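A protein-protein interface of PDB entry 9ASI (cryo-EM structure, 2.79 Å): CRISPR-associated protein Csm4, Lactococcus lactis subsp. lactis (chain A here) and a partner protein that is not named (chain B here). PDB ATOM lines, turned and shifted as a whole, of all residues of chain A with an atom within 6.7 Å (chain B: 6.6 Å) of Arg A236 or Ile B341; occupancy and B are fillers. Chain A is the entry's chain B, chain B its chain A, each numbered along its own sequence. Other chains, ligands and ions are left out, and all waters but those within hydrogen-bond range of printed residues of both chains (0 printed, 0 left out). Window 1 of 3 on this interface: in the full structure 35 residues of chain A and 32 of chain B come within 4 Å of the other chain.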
ATOM      1  N   GLU A  16     -22.771   6.050  12.907  1.00  0.00           N
ATOM      2  CA  GLU A  16     -23.233   4.683  12.703  1.00  0.00           C
ATOM      3  C   GLU A  16     -22.185   3.649  13.096  1.00  0.00           C
ATOM      4  O   GLU A  16     -22.505   2.676  13.783  1.00  0.00           O
ATOM      5  CB  GLU A  16     -23.669   4.497  11.240  1.00  0.00           C
ATOM      6  CG  GLU A  16     -22.551   4.492  10.191  1.00  0.00           C
ATOM      7  CD  GLU A  16     -21.902   5.855   9.966  1.00  0.00           C
ATOM      8  OE1 GLU A  16     -22.143   6.788  10.757  1.00  0.00           O
ATOM      9  OE2 GLU A  16     -21.135   5.989   8.991  1.00  0.00           O
ATOM     10  N   LYS A  17     -20.936   3.826  12.666  1.00  0.00           N
ATOM     11  CA  LYS A  17     -19.852   2.961  13.118  1.00  0.00           C
ATOM     12  C   LYS A  17     -18.569   3.698  13.472  1.00  0.00           C
ATOM     13  O   LYS A  17     -17.769   3.154  14.240  1.00  0.00           O
ATOM     14  CB  LYS A  17     -19.542   1.895  12.060  1.00  0.00           C
ATOM     15  CG  LYS A  17     -18.774   0.693  12.582  1.00  0.00           C
ATOM     16  CD  LYS A  17     -18.855  -0.465  11.610  1.00  0.00           C
ATOM     17  CE  LYS A  17     -18.225  -0.105  10.279  1.00  0.00           C
ATOM     18  NZ  LYS A  17     -18.294  -1.232   9.312  1.00  0.00           N
ATOM     19  N   LEU A 233     -35.090  -5.539   6.634  1.00  0.00           N
ATOM     20  CA  LEU A 233     -33.658  -5.321   6.486  1.00  0.00           C
ATOM     21  C   LEU A 233     -33.036  -5.297   7.873  1.00  0.00           C
ATOM     22  O   LEU A 233     -33.515  -4.574   8.751  1.00  0.00           O
ATOM     23  CB  LEU A 233     -33.371  -4.012   5.746  1.00  0.00           C
ATOM     24  CG  LEU A 233     -32.096  -3.958   4.908  1.00  0.00           C
ATOM     25  CD1 LEU A 233     -32.249  -4.803   3.659  1.00  0.00           C
ATOM     26  CD2 LEU A 233     -31.764  -2.523   4.547  1.00  0.00           C
ATOM     27  N   LEU A 234     -31.985  -6.086   8.067  1.00  0.00           N
ATOM     28  CA  LEU A 234     -31.300  -6.159   9.348  1.00  0.00           C
ATOM     29  C   LEU A 234     -30.248  -5.063   9.466  1.00  0.00           C
ATOM     30  O   LEU A 234     -29.805  -4.476   8.476  1.00  0.00           O
ATOM     31  CB  LEU A 234     -30.634  -7.520   9.537  1.00  0.00           C
ATOM     32  CG  LEU A 234     -31.505  -8.765   9.660  1.00  0.00           C
ATOM     33  CD1 LEU A 234     -30.631  -9.973   9.916  1.00  0.00           C
ATOM     34  CD2 LEU A 234     -32.489  -8.598  10.779  1.00  0.00           C
ATOM     35  N   GLU A 235     -29.848  -4.797  10.705  1.00  0.00           N
ATOM     36  CA  GLU A 235     -28.803  -3.830  10.997  1.00  0.00           C
ATOM     37  C   GLU A 235     -28.201  -4.175  12.349  1.00  0.00           C
ATOM     38  O   GLU A 235     -28.931  -4.493  13.289  1.00  0.00           O
ATOM     39  CB  GLU A 235     -29.349  -2.399  11.000  1.00  0.00           C
ATOM     40  CG  GLU A 235     -30.667  -2.244  11.725  1.00  0.00           C
ATOM     41  CD  GLU A 235     -31.025  -0.793  11.958  1.00  0.00           C
ATOM     42  OE1 GLU A 235     -30.263   0.082  11.498  1.00  0.00           O
ATOM     43  OE2 GLU A 235     -32.064  -0.527  12.597  1.00  0.00           O
ATOM     44  N   ARG A 236     -26.877  -4.115  12.445  1.00  0.00           N
ATOM     45  CA  ARG A 236     -26.214  -4.454  13.694  1.00  0.00           C
ATOM     46  C   ARG A 236     -26.245  -3.260  14.634  1.00  0.00           C
ATOM     47  O   ARG A 236     -25.858  -2.149  14.260  1.00  0.00           O
ATOM     48  CB  ARG A 236     -24.775  -4.907  13.445  1.00  0.00           C
ATOM     49  CG  ARG A 236     -23.949  -3.977  12.582  1.00  0.00           C
ATOM     50  CD  ARG A 236     -22.468  -4.285  12.716  1.00  0.00           C
ATOM     51  NE  ARG A 236     -22.045  -4.330  14.110  1.00  0.00           N
ATOM     52  CZ  ARG A 236     -21.843  -3.261  14.868  1.00  0.00           C
ATOM     53  NH1 ARG A 236     -22.030  -2.039  14.403  1.00  0.00           N
ATOM     54  NH2 ARG A 236     -21.443  -3.424  16.125  1.00  0.00           N
ATOM     55  N   ARG A 237     -26.726  -3.489  15.851  1.00  0.00           N
ATOM     56  CA  ARG A 237     -26.810  -2.466  16.889  1.00  0.00           C
ATOM     57  C   ARG A 237     -25.860  -2.887  18.004  1.00  0.00           C
ATOM     58  O   ARG A 237     -26.250  -3.573  18.948  1.00  0.00           O
ATOM     59  CB  ARG A 237     -28.238  -2.301  17.410  1.00  0.00           C
ATOM     60  CG  ARG A 237     -29.313  -2.095  16.355  1.00  0.00           C
ATOM     61  CD  ARG A 237     -28.847  -1.254  15.181  1.00  0.00           C
ATOM     62  NE  ARG A 237     -28.660   0.143  15.545  1.00  0.00           N
ATOM     63  CZ  ARG A 237     -29.644   1.022  15.660  1.00  0.00           C
ATOM     64  NH1 ARG A 237     -30.904   0.680  15.444  1.00  0.00           N
ATOM     65  NH2 ARG A 237     -29.358   2.274  16.006  1.00  0.00           N
ATOM     66  N   GLY A 238     -24.612  -2.471  17.890  1.00  0.00           N
ATOM     67  CA  GLY A 238     -23.608  -2.774  18.892  1.00  0.00           C
ATOM     68  C   GLY A 238     -22.866  -1.518  19.291  1.00  0.00           C
ATOM     69  O   GLY A 238     -23.443  -0.442  19.437  1.00  0.00           O
ATOM     70  N   GLY A 239     -21.559  -1.669  19.460  1.00  0.00           N
ATOM     71  CA  GLY A 239     -20.714  -0.563  19.850  1.00  0.00           C
ATOM     72  C   GLY A 239     -20.162  -0.754  21.241  1.00  0.00           C
ATOM     73  O   GLY A 239     -19.996  -1.886  21.698  1.00  0.00           O
ATOM     74  N   LYS A 252     -16.879  -3.564  24.592  1.00  0.00           N
ATOM     75  CA  LYS A 252     -17.991  -3.567  23.657  1.00  0.00           C
ATOM     76  C   LYS A 252     -19.148  -4.397  24.206  1.00  0.00           C
ATOM     77  O   LYS A 252     -19.035  -5.087  25.222  1.00  0.00           O
ATOM     78  CB  LYS A 252     -17.563  -4.114  22.299  1.00  0.00           C
ATOM     79  CG  LYS A 252     -16.713  -3.177  21.486  1.00  0.00           C
ATOM     80  CD  LYS A 252     -16.151  -3.881  20.276  1.00  0.00           C
ATOM     81  CE  LYS A 252     -17.195  -4.047  19.199  1.00  0.00           C
ATOM     82  NZ  LYS A 252     -17.438  -2.781  18.482  1.00  0.00           N
ATOM     83  N   LYS A 253     -20.276  -4.327  23.509  1.00  0.00           N
ATOM     84  CA  LYS A 253     -21.473  -5.059  23.880  1.00  0.00           C
ATOM     85  C   LYS A 253     -21.859  -6.024  22.766  1.00  0.00           C
ATOM     86  O   LYS A 253     -21.390  -5.916  21.629  1.00  0.00           O
ATOM     87  CB  LYS A 253     -22.630  -4.103  24.190  1.00  0.00           C
ATOM     88  CG  LYS A 253     -23.393  -3.625  22.977  1.00  0.00           C
ATOM     89  CD  LYS A 253     -24.344  -2.506  23.347  1.00  0.00           C
ATOM     90  CE  LYS A 253     -23.606  -1.199  23.524  1.00  0.00           C
ATOM     91  NZ  LYS A 253     -24.468  -0.024  23.241  1.00  0.00           N
ATOM     92  N   ASP A 255     -23.382  -7.501  19.807  1.00  0.00           N
ATOM     93  CA  ASP A 255     -24.040  -6.914  18.649  1.00  0.00           C
ATOM     94  C   ASP A 255     -25.417  -7.531  18.462  1.00  0.00           C
ATOM     95  O   ASP A 255     -25.573  -8.755  18.485  1.00  0.00           O
ATOM     96  CB  ASP A 255     -23.194  -7.114  17.393  1.00  0.00           C
ATOM     97  CG  ASP A 255     -21.910  -6.309  17.420  1.00  0.00           C
ATOM     98  OD1 ASP A 255     -21.730  -5.495  18.349  1.00  0.00           O
ATOM     99  OD2 ASP A 255     -21.082  -6.480  16.503  1.00  0.00           O
ATOM    100  N   LEU A 256     -26.416  -6.680  18.283  1.00  0.00           N
ATOM    101  CA  LEU A 256     -27.788  -7.113  18.081  1.00  0.00           C
ATOM    102  C   LEU A 256     -28.222  -6.747  16.673  1.00  0.00           C
ATOM    103  O   LEU A 256     -27.942  -5.645  16.195  1.00  0.00           O
ATOM    104  CB  LEU A 256     -28.727  -6.474  19.108  1.00  0.00           C
ATOM    105  CG  LEU A 256     -30.092  -7.136  19.293  1.00  0.00           C
ATOM    106  CD1 LEU A 256     -29.988  -8.303  20.253  1.00  0.00           C
ATOM    107  CD2 LEU A 256     -31.099  -6.129  19.795  1.00  0.00           C
ATOM    108  N   TYR A 257     -28.896  -7.675  16.009  1.00  0.00           N
ATOM    109  CA  TYR A 257     -29.357  -7.475  14.645  1.00  0.00           C
ATOM    110  C   TYR A 257     -30.871  -7.338  14.667  1.00  0.00           C
ATOM    111  O   TYR A 257     -31.577  -8.260  15.088  1.00  0.00           O
ATOM    112  CB  TYR A 257     -28.903  -8.626  13.748  1.00  0.00           C
ATOM    113  CG  TYR A 257     -27.399  -8.676  13.594  1.00  0.00           C
ATOM    114  CD1 TYR A 257     -26.601  -9.252  14.571  1.00  0.00           C
ATOM    115  CD2 TYR A 257     -26.777  -8.131  12.483  1.00  0.00           C
ATOM    116  CE1 TYR A 257     -25.231  -9.289  14.443  1.00  0.00           C
ATOM    117  CE2 TYR A 257     -25.406  -8.166  12.345  1.00  0.00           C
ATOM    118  CZ  TYR A 257     -24.640  -8.745  13.329  1.00  0.00           C
ATOM    119  OH  TYR A 257     -23.271  -8.784  13.202  1.00  0.00           O
ATOM    120  N   VAL A 258     -31.364  -6.185  14.220  1.00  0.00           N
ATOM    121  CA  VAL A 258     -32.768  -5.833  14.336  1.00  0.00           C
ATOM    122  C   VAL A 258     -33.291  -5.414  12.972  1.00  0.00           C
ATOM    123  O   VAL A 258     -32.539  -4.989  12.094  1.00  0.00           O
ATOM    124  CB  VAL A 258     -32.995  -4.697  15.352  1.00  0.00           C
ATOM    125  CG1 VAL A 258     -32.623  -5.145  16.741  1.00  0.00           C
ATOM    126  CG2 VAL A 258     -32.201  -3.478  14.951  1.00  0.00           C
ATOM    127  N   SER B 255     -24.472  -7.931  -2.566  1.00  0.00           N
ATOM    128  CA  SER B 255     -25.078  -6.758  -1.954  1.00  0.00           C
ATOM    129  C   SER B 255     -24.160  -6.187  -0.884  1.00  0.00           C
ATOM    130  O   SER B 255     -23.517  -6.932  -0.139  1.00  0.00           O
ATOM    131  CB  SER B 255     -26.437  -7.104  -1.340  1.00  0.00           C
ATOM    132  OG  SER B 255     -27.335  -7.594  -2.319  1.00  0.00           O
ATOM    133  N   GLY B 256     -24.108  -4.861  -0.808  1.00  0.00           N
ATOM    134  CA  GLY B 256     -23.287  -4.199   0.184  1.00  0.00           C
ATOM    135  C   GLY B 256     -21.809  -4.176  -0.124  1.00  0.00           C
ATOM    136  O   GLY B 256     -20.993  -4.168   0.802  1.00  0.00           O
ATOM    137  N   PHE B 335     -21.103 -16.889   3.890  1.00  0.00           N
ATOM    138  CA  PHE B 335     -21.096 -15.433   3.952  1.00  0.00           C
ATOM    139  C   PHE B 335     -21.492 -14.944   5.336  1.00  0.00           C
ATOM    140  O   PHE B 335     -20.885 -14.007   5.862  1.00  0.00           O
ATOM    141  CB  PHE B 335     -22.012 -14.857   2.876  1.00  0.00           C
ATOM    142  CG  PHE B 335     -21.313 -14.576   1.573  1.00  0.00           C
ATOM    143  CD1 PHE B 335     -20.481 -13.481   1.441  1.00  0.00           C
ATOM    144  CD2 PHE B 335     -21.483 -15.413   0.486  1.00  0.00           C
ATOM    145  CE1 PHE B 335     -19.838 -13.222   0.249  1.00  0.00           C
ATOM    146  CE2 PHE B 335     -20.840 -15.158  -0.708  1.00  0.00           C
ATOM    147  CZ  PHE B 335     -20.019 -14.061  -0.826  1.00  0.00           C
ATOM    148  N   LEU B 336     -22.490 -15.582   5.955  1.00  0.00           N
ATOM    149  CA  LEU B 336     -22.833 -15.273   7.340  1.00  0.00           C
ATOM    150  C   LEU B 336     -21.632 -15.460   8.255  1.00  0.00           C
ATOM    151  O   LEU B 336     -21.391 -14.645   9.152  1.00  0.00           O
ATOM    152  CB  LEU B 336     -23.981 -16.165   7.811  1.00  0.00           C
ATOM    153  CG  LEU B 336     -25.435 -15.812   7.510  1.00  0.00           C
ATOM    154  CD1 LEU B 336     -26.332 -16.746   8.293  1.00  0.00           C
ATOM    155  CD2 LEU B 336     -25.743 -14.376   7.859  1.00  0.00           C
ATOM    156  N   PHE B 339     -18.957 -12.463   6.572  1.00  0.00           N
ATOM    157  CA  PHE B 339     -19.575 -11.137   6.573  1.00  0.00           C
ATOM    158  C   PHE B 339     -20.978 -11.296   7.150  1.00  0.00           C
ATOM    159  O   PHE B 339     -21.901 -11.697   6.436  1.00  0.00           O
ATOM    160  CB  PHE B 339     -19.631 -10.550   5.166  1.00  0.00           C
ATOM    161  CG  PHE B 339     -18.363 -10.713   4.385  1.00  0.00           C
ATOM    162  CD1 PHE B 339     -17.263  -9.916   4.644  1.00  0.00           C
ATOM    163  CD2 PHE B 339     -18.275 -11.662   3.383  1.00  0.00           C
ATOM    164  CE1 PHE B 339     -16.099 -10.066   3.919  1.00  0.00           C
ATOM    165  CE2 PHE B 339     -17.114 -11.817   2.657  1.00  0.00           C
ATOM    166  CZ  PHE B 339     -16.024 -11.017   2.924  1.00  0.00           C
ATOM    167  N   LYS B 340     -21.139 -10.963   8.431  1.00  0.00           N
ATOM    168  CA  LYS B 340     -22.382 -11.267   9.136  1.00  0.00           C
ATOM    169  C   LYS B 340     -23.597 -10.785   8.353  1.00  0.00           C
ATOM    170  O   LYS B 340     -24.425 -11.585   7.908  1.00  0.00           O
ATOM    171  CB  LYS B 340     -22.344 -10.644  10.531  1.00  0.00           C
ATOM    172  CG  LYS B 340     -20.973 -10.704  11.184  1.00  0.00           C
ATOM    173  CD  LYS B 340     -20.513 -12.137  11.389  1.00  0.00           C
ATOM    174  CE  LYS B 340     -21.430 -12.879  12.338  1.00  0.00           C
ATOM    175  NZ  LYS B 340     -21.469 -12.229  13.674  1.00  0.00           N
ATOM    176  N   ILE B 341     -23.709  -9.471   8.152  1.00  0.00           N
ATOM    177  CA  ILE B 341     -24.642  -8.905   7.187  1.00  0.00           C
ATOM    178  C   ILE B 341     -23.994  -7.834   6.328  1.00  0.00           C
ATOM    179  O   ILE B 341     -24.673  -7.227   5.499  1.00  0.00           O
ATOM    180  CB  ILE B 341     -25.910  -8.340   7.863  1.00  0.00           C
ATOM    181  CG1 ILE B 341     -25.546  -7.199   8.815  1.00  0.00           C
ATOM    182  CG2 ILE B 341     -26.692  -9.435   8.572  1.00  0.00           C
ATOM    183  CD1 ILE B 341     -26.735  -6.447   9.333  1.00  0.00           C
ATOM    184  N   ASP B 342     -22.697  -7.582   6.503  1.00  0.00           N
ATOM    185  CA  ASP B 342     -22.014  -6.523   5.777  1.00  0.00           C
ATOM    186  C   ASP B 342     -21.758  -6.881   4.324  1.00  0.00           C
ATOM    187  O   ASP B 342     -21.324  -6.015   3.557  1.00  0.00           O
ATOM    188  CB  ASP B 342     -20.700  -6.187   6.481  1.00  0.00           C
ATOM    189  CG  ASP B 342     -20.918  -5.463   7.795  1.00  0.00           C
ATOM    190  OD1 ASP B 342     -21.048  -4.221   7.782  1.00  0.00           O
ATOM    191  OD2 ASP B 342     -20.977  -6.139   8.843  1.00  0.00           O
ATOM    192  N   LEU B 343     -22.017  -8.124   3.931  1.00  0.00           N
ATOM    193  CA  LEU B 343     -21.909  -8.534   2.541  1.00  0.00           C
ATOM    194  C   LEU B 343     -22.763  -9.776   2.353  1.00  0.00           C
ATOM    195  O   LEU B 343     -22.788 -10.652   3.218  1.00  0.00           O
ATOM    196  CB  LEU B 343     -20.457  -8.815   2.148  1.00  0.00           C
ATOM    197  CG  LEU B 343     -20.163  -8.767   0.654  1.00  0.00           C
ATOM    198  CD1 LEU B 343     -20.241  -7.341   0.169  1.00  0.00           C
ATOM    199  CD2 LEU B 343     -18.806  -9.358   0.373  1.00  0.00           C
ATOM    200  N   TYR B 344     -23.455  -9.843   1.220  1.00  0.00           N
ATOM    201  CA  TYR B 344     -24.429 -10.898   0.994  1.00  0.00           C
ATOM    202  C   TYR B 344     -24.697 -11.002  -0.498  1.00  0.00           C
ATOM    203  O   TYR B 344     -24.809  -9.983  -1.184  1.00  0.00           O
ATOM    204  CB  TYR B 344     -25.726 -10.607   1.760  1.00  0.00           C
ATOM    205  CG  TYR B 344     -26.904 -11.482   1.402  1.00  0.00           C
ATOM    206  CD1 TYR B 344     -27.053 -12.741   1.964  1.00  0.00           C
ATOM    207  CD2 TYR B 344     -27.881 -11.037   0.527  1.00  0.00           C
ATOM    208  CE1 TYR B 344     -28.133 -13.536   1.651  1.00  0.00           C
ATOM    209  CE2 TYR B 344     -28.963 -11.826   0.207  1.00  0.00           C
ATOM    210  CZ  TYR B 344     -29.083 -13.074   0.770  1.00  0.00           C
ATOM    211  OH  TYR B 344     -30.165 -13.861   0.453  1.00  0.00           O
ATOM    212  N   ARG B 382     -34.230 -11.776   3.373  1.00  0.00           N
ATOM    213  CA  ARG B 382     -32.927 -12.369   3.083  1.00  0.00           C
ATOM    214  C   ARG B 382     -32.672 -13.627   3.900  1.00  0.00           C
ATOM    215  O   ARG B 382     -32.090 -14.592   3.393  1.00  0.00           O
ATOM    216  CB  ARG B 382     -31.823 -11.345   3.332  1.00  0.00           C
ATOM    217  CG  ARG B 382     -31.568 -10.419   2.168  1.00  0.00           C
ATOM    218  CD  ARG B 382     -30.470  -9.429   2.493  1.00  0.00           C
ATOM    219  NE  ARG B 382     -30.579  -8.220   1.690  1.00  0.00           N
ATOM    220  CZ  ARG B 382     -29.579  -7.379   1.468  1.00  0.00           C
ATOM    221  NH1 ARG B 382     -28.378  -7.586   1.984  1.00  0.00           N
ATOM    222  NH2 ARG B 382     -29.789  -6.303   0.716  1.00  0.00           N
ATOM    223  N   TYR B 383     -33.092 -13.643   5.160  1.00  0.00           N
ATOM    224  CA  TYR B 383     -32.679 -14.681   6.090  1.00  0.00           C
ATOM    225  C   TYR B 383     -33.889 -15.296   6.776  1.00  0.00           C
ATOM    226  O   TYR B 383     -34.907 -14.634   6.993  1.00  0.00           O
ATOM    227  CB  TYR B 383     -31.705 -14.114   7.129  1.00  0.00           C
ATOM    228  CG  TYR B 383     -30.673 -13.190   6.526  1.00  0.00           C
ATOM    229  CD1 TYR B 383     -29.720 -13.668   5.639  1.00  0.00           C
ATOM    230  CD2 TYR B 383     -30.662 -11.836   6.825  1.00  0.00           C
ATOM    231  CE1 TYR B 383     -28.778 -12.830   5.078  1.00  0.00           C
ATOM    232  CE2 TYR B 383     -29.725 -10.989   6.266  1.00  0.00           C
ATOM    233  CZ  TYR B 383     -28.786 -11.492   5.393  1.00  0.00           C
ATOM    234  OH  TYR B 383     -27.848 -10.657   4.837  1.00  0.00           O
ATOM    235  N   LEU B 391     -27.278 -15.255  14.427  1.00  0.00           N
ATOM    236  CA  LEU B 391     -26.592 -13.968  14.436  1.00  0.00           C
ATOM    237  C   LEU B 391     -26.659 -13.317  15.808  1.00  0.00           C
ATOM    238  O   LEU B 391     -25.664 -12.769  16.294  1.00  0.00           O
ATOM    239  CB  LEU B 391     -27.204 -13.047  13.384  1.00  0.00           C
ATOM    240  CG  LEU B 391     -26.548 -13.023  12.008  1.00  0.00           C
ATOM    241  CD1 LEU B 391     -27.258 -12.019  11.125  1.00  0.00           C
ATOM    242  CD2 LEU B 391     -25.081 -12.678  12.136  1.00  0.00           C
ATOM    243  N   LYS B 406     -13.718  -3.050  12.107  1.00  0.00           N
ATOM    244  CA  LYS B 406     -14.394  -2.775  13.380  1.00  0.00           C
ATOM    245  C   LYS B 406     -15.247  -3.950  13.853  1.00  0.00           C
ATOM    246  O   LYS B 406     -16.309  -3.773  14.450  1.00  0.00           O
ATOM    247  CB  LYS B 406     -15.237  -1.504  13.292  1.00  0.00           C
ATOM    248  CG  LYS B 406     -14.436  -0.229  13.416  1.00  0.00           C
ATOM    249  CD  LYS B 406     -15.322   0.942  13.769  1.00  0.00           C
ATOM    250  CE  LYS B 406     -14.512   2.214  13.865  1.00  0.00           C
ATOM    251  NZ  LYS B 406     -13.524   2.140  14.971  1.00  0.00           N
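The side-chain carboxylate (OE2) of Glu A235 lies within salt-bridge range of the guanidinium group (NH1) of Arg A237, at 3.3 Å. N of Glu A235 lies within hydrogen-bond range of O of Val A258 (3.0 Å). NH2 of Arg A236 is in salt-bridge range of OD1 of Asp A255, 3.1 Å away.
Among the printed residues, pairs that only touch across the chains: Lys A17 with Lys B406 (3.3 Å), Leu A234 with Ile B341 (3.7 Å), Leu A234 with Tyr B383 (3.6 Å), Glu A235 with Ile B341 (3.7 Å), Arg A236 with Ile B341 (3.9 Å), Tyr A257 with Lys B340 (3.4 Å), Tyr A257 with Ile B341 (3.6 Å) and Tyr A257 with Leu B391 (3.97 Å).
Arg A236 touches just one residue of chain B: Ile B341. Ile B341 touches just these residues of chain A: Leu A234 (3.7 Å), Glu A235 (3.7 Å), Arg A236 (3.9 Å) and Tyr A257 (3.6 Å). Of the printed residues of chain A, Lys B340 touches Tyr A257 (3.4 Å). Printed residues of chain A within 4 Å of Leu B391: Tyr A257 (3.97 Å). Of the printed residues of chain B, Leu A234 touches Ile B341 and Tyr B383. Of the printed residues of chain B, Glu A235 touches Ile B341. Asp B342 touches none of the printed residues of chain A. The nearest residue of chain B that does not touch Arg A236 is Asp B342 (4.5 Å). The nearest printed residue of chain A that does not touch Tyr B383 is Leu A233 (6.8 Å).
Hydrophobic or aromatic side chains of chain B that line the printed part of chain A: Ile B341 and Tyr B383. Among the printed residues, 8 pairs touch across the chains. Among the printed residues, no Asp or Glu carboxylate lies within 4 Å of a Lys or Arg side-chain nitrogen of the other chain.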
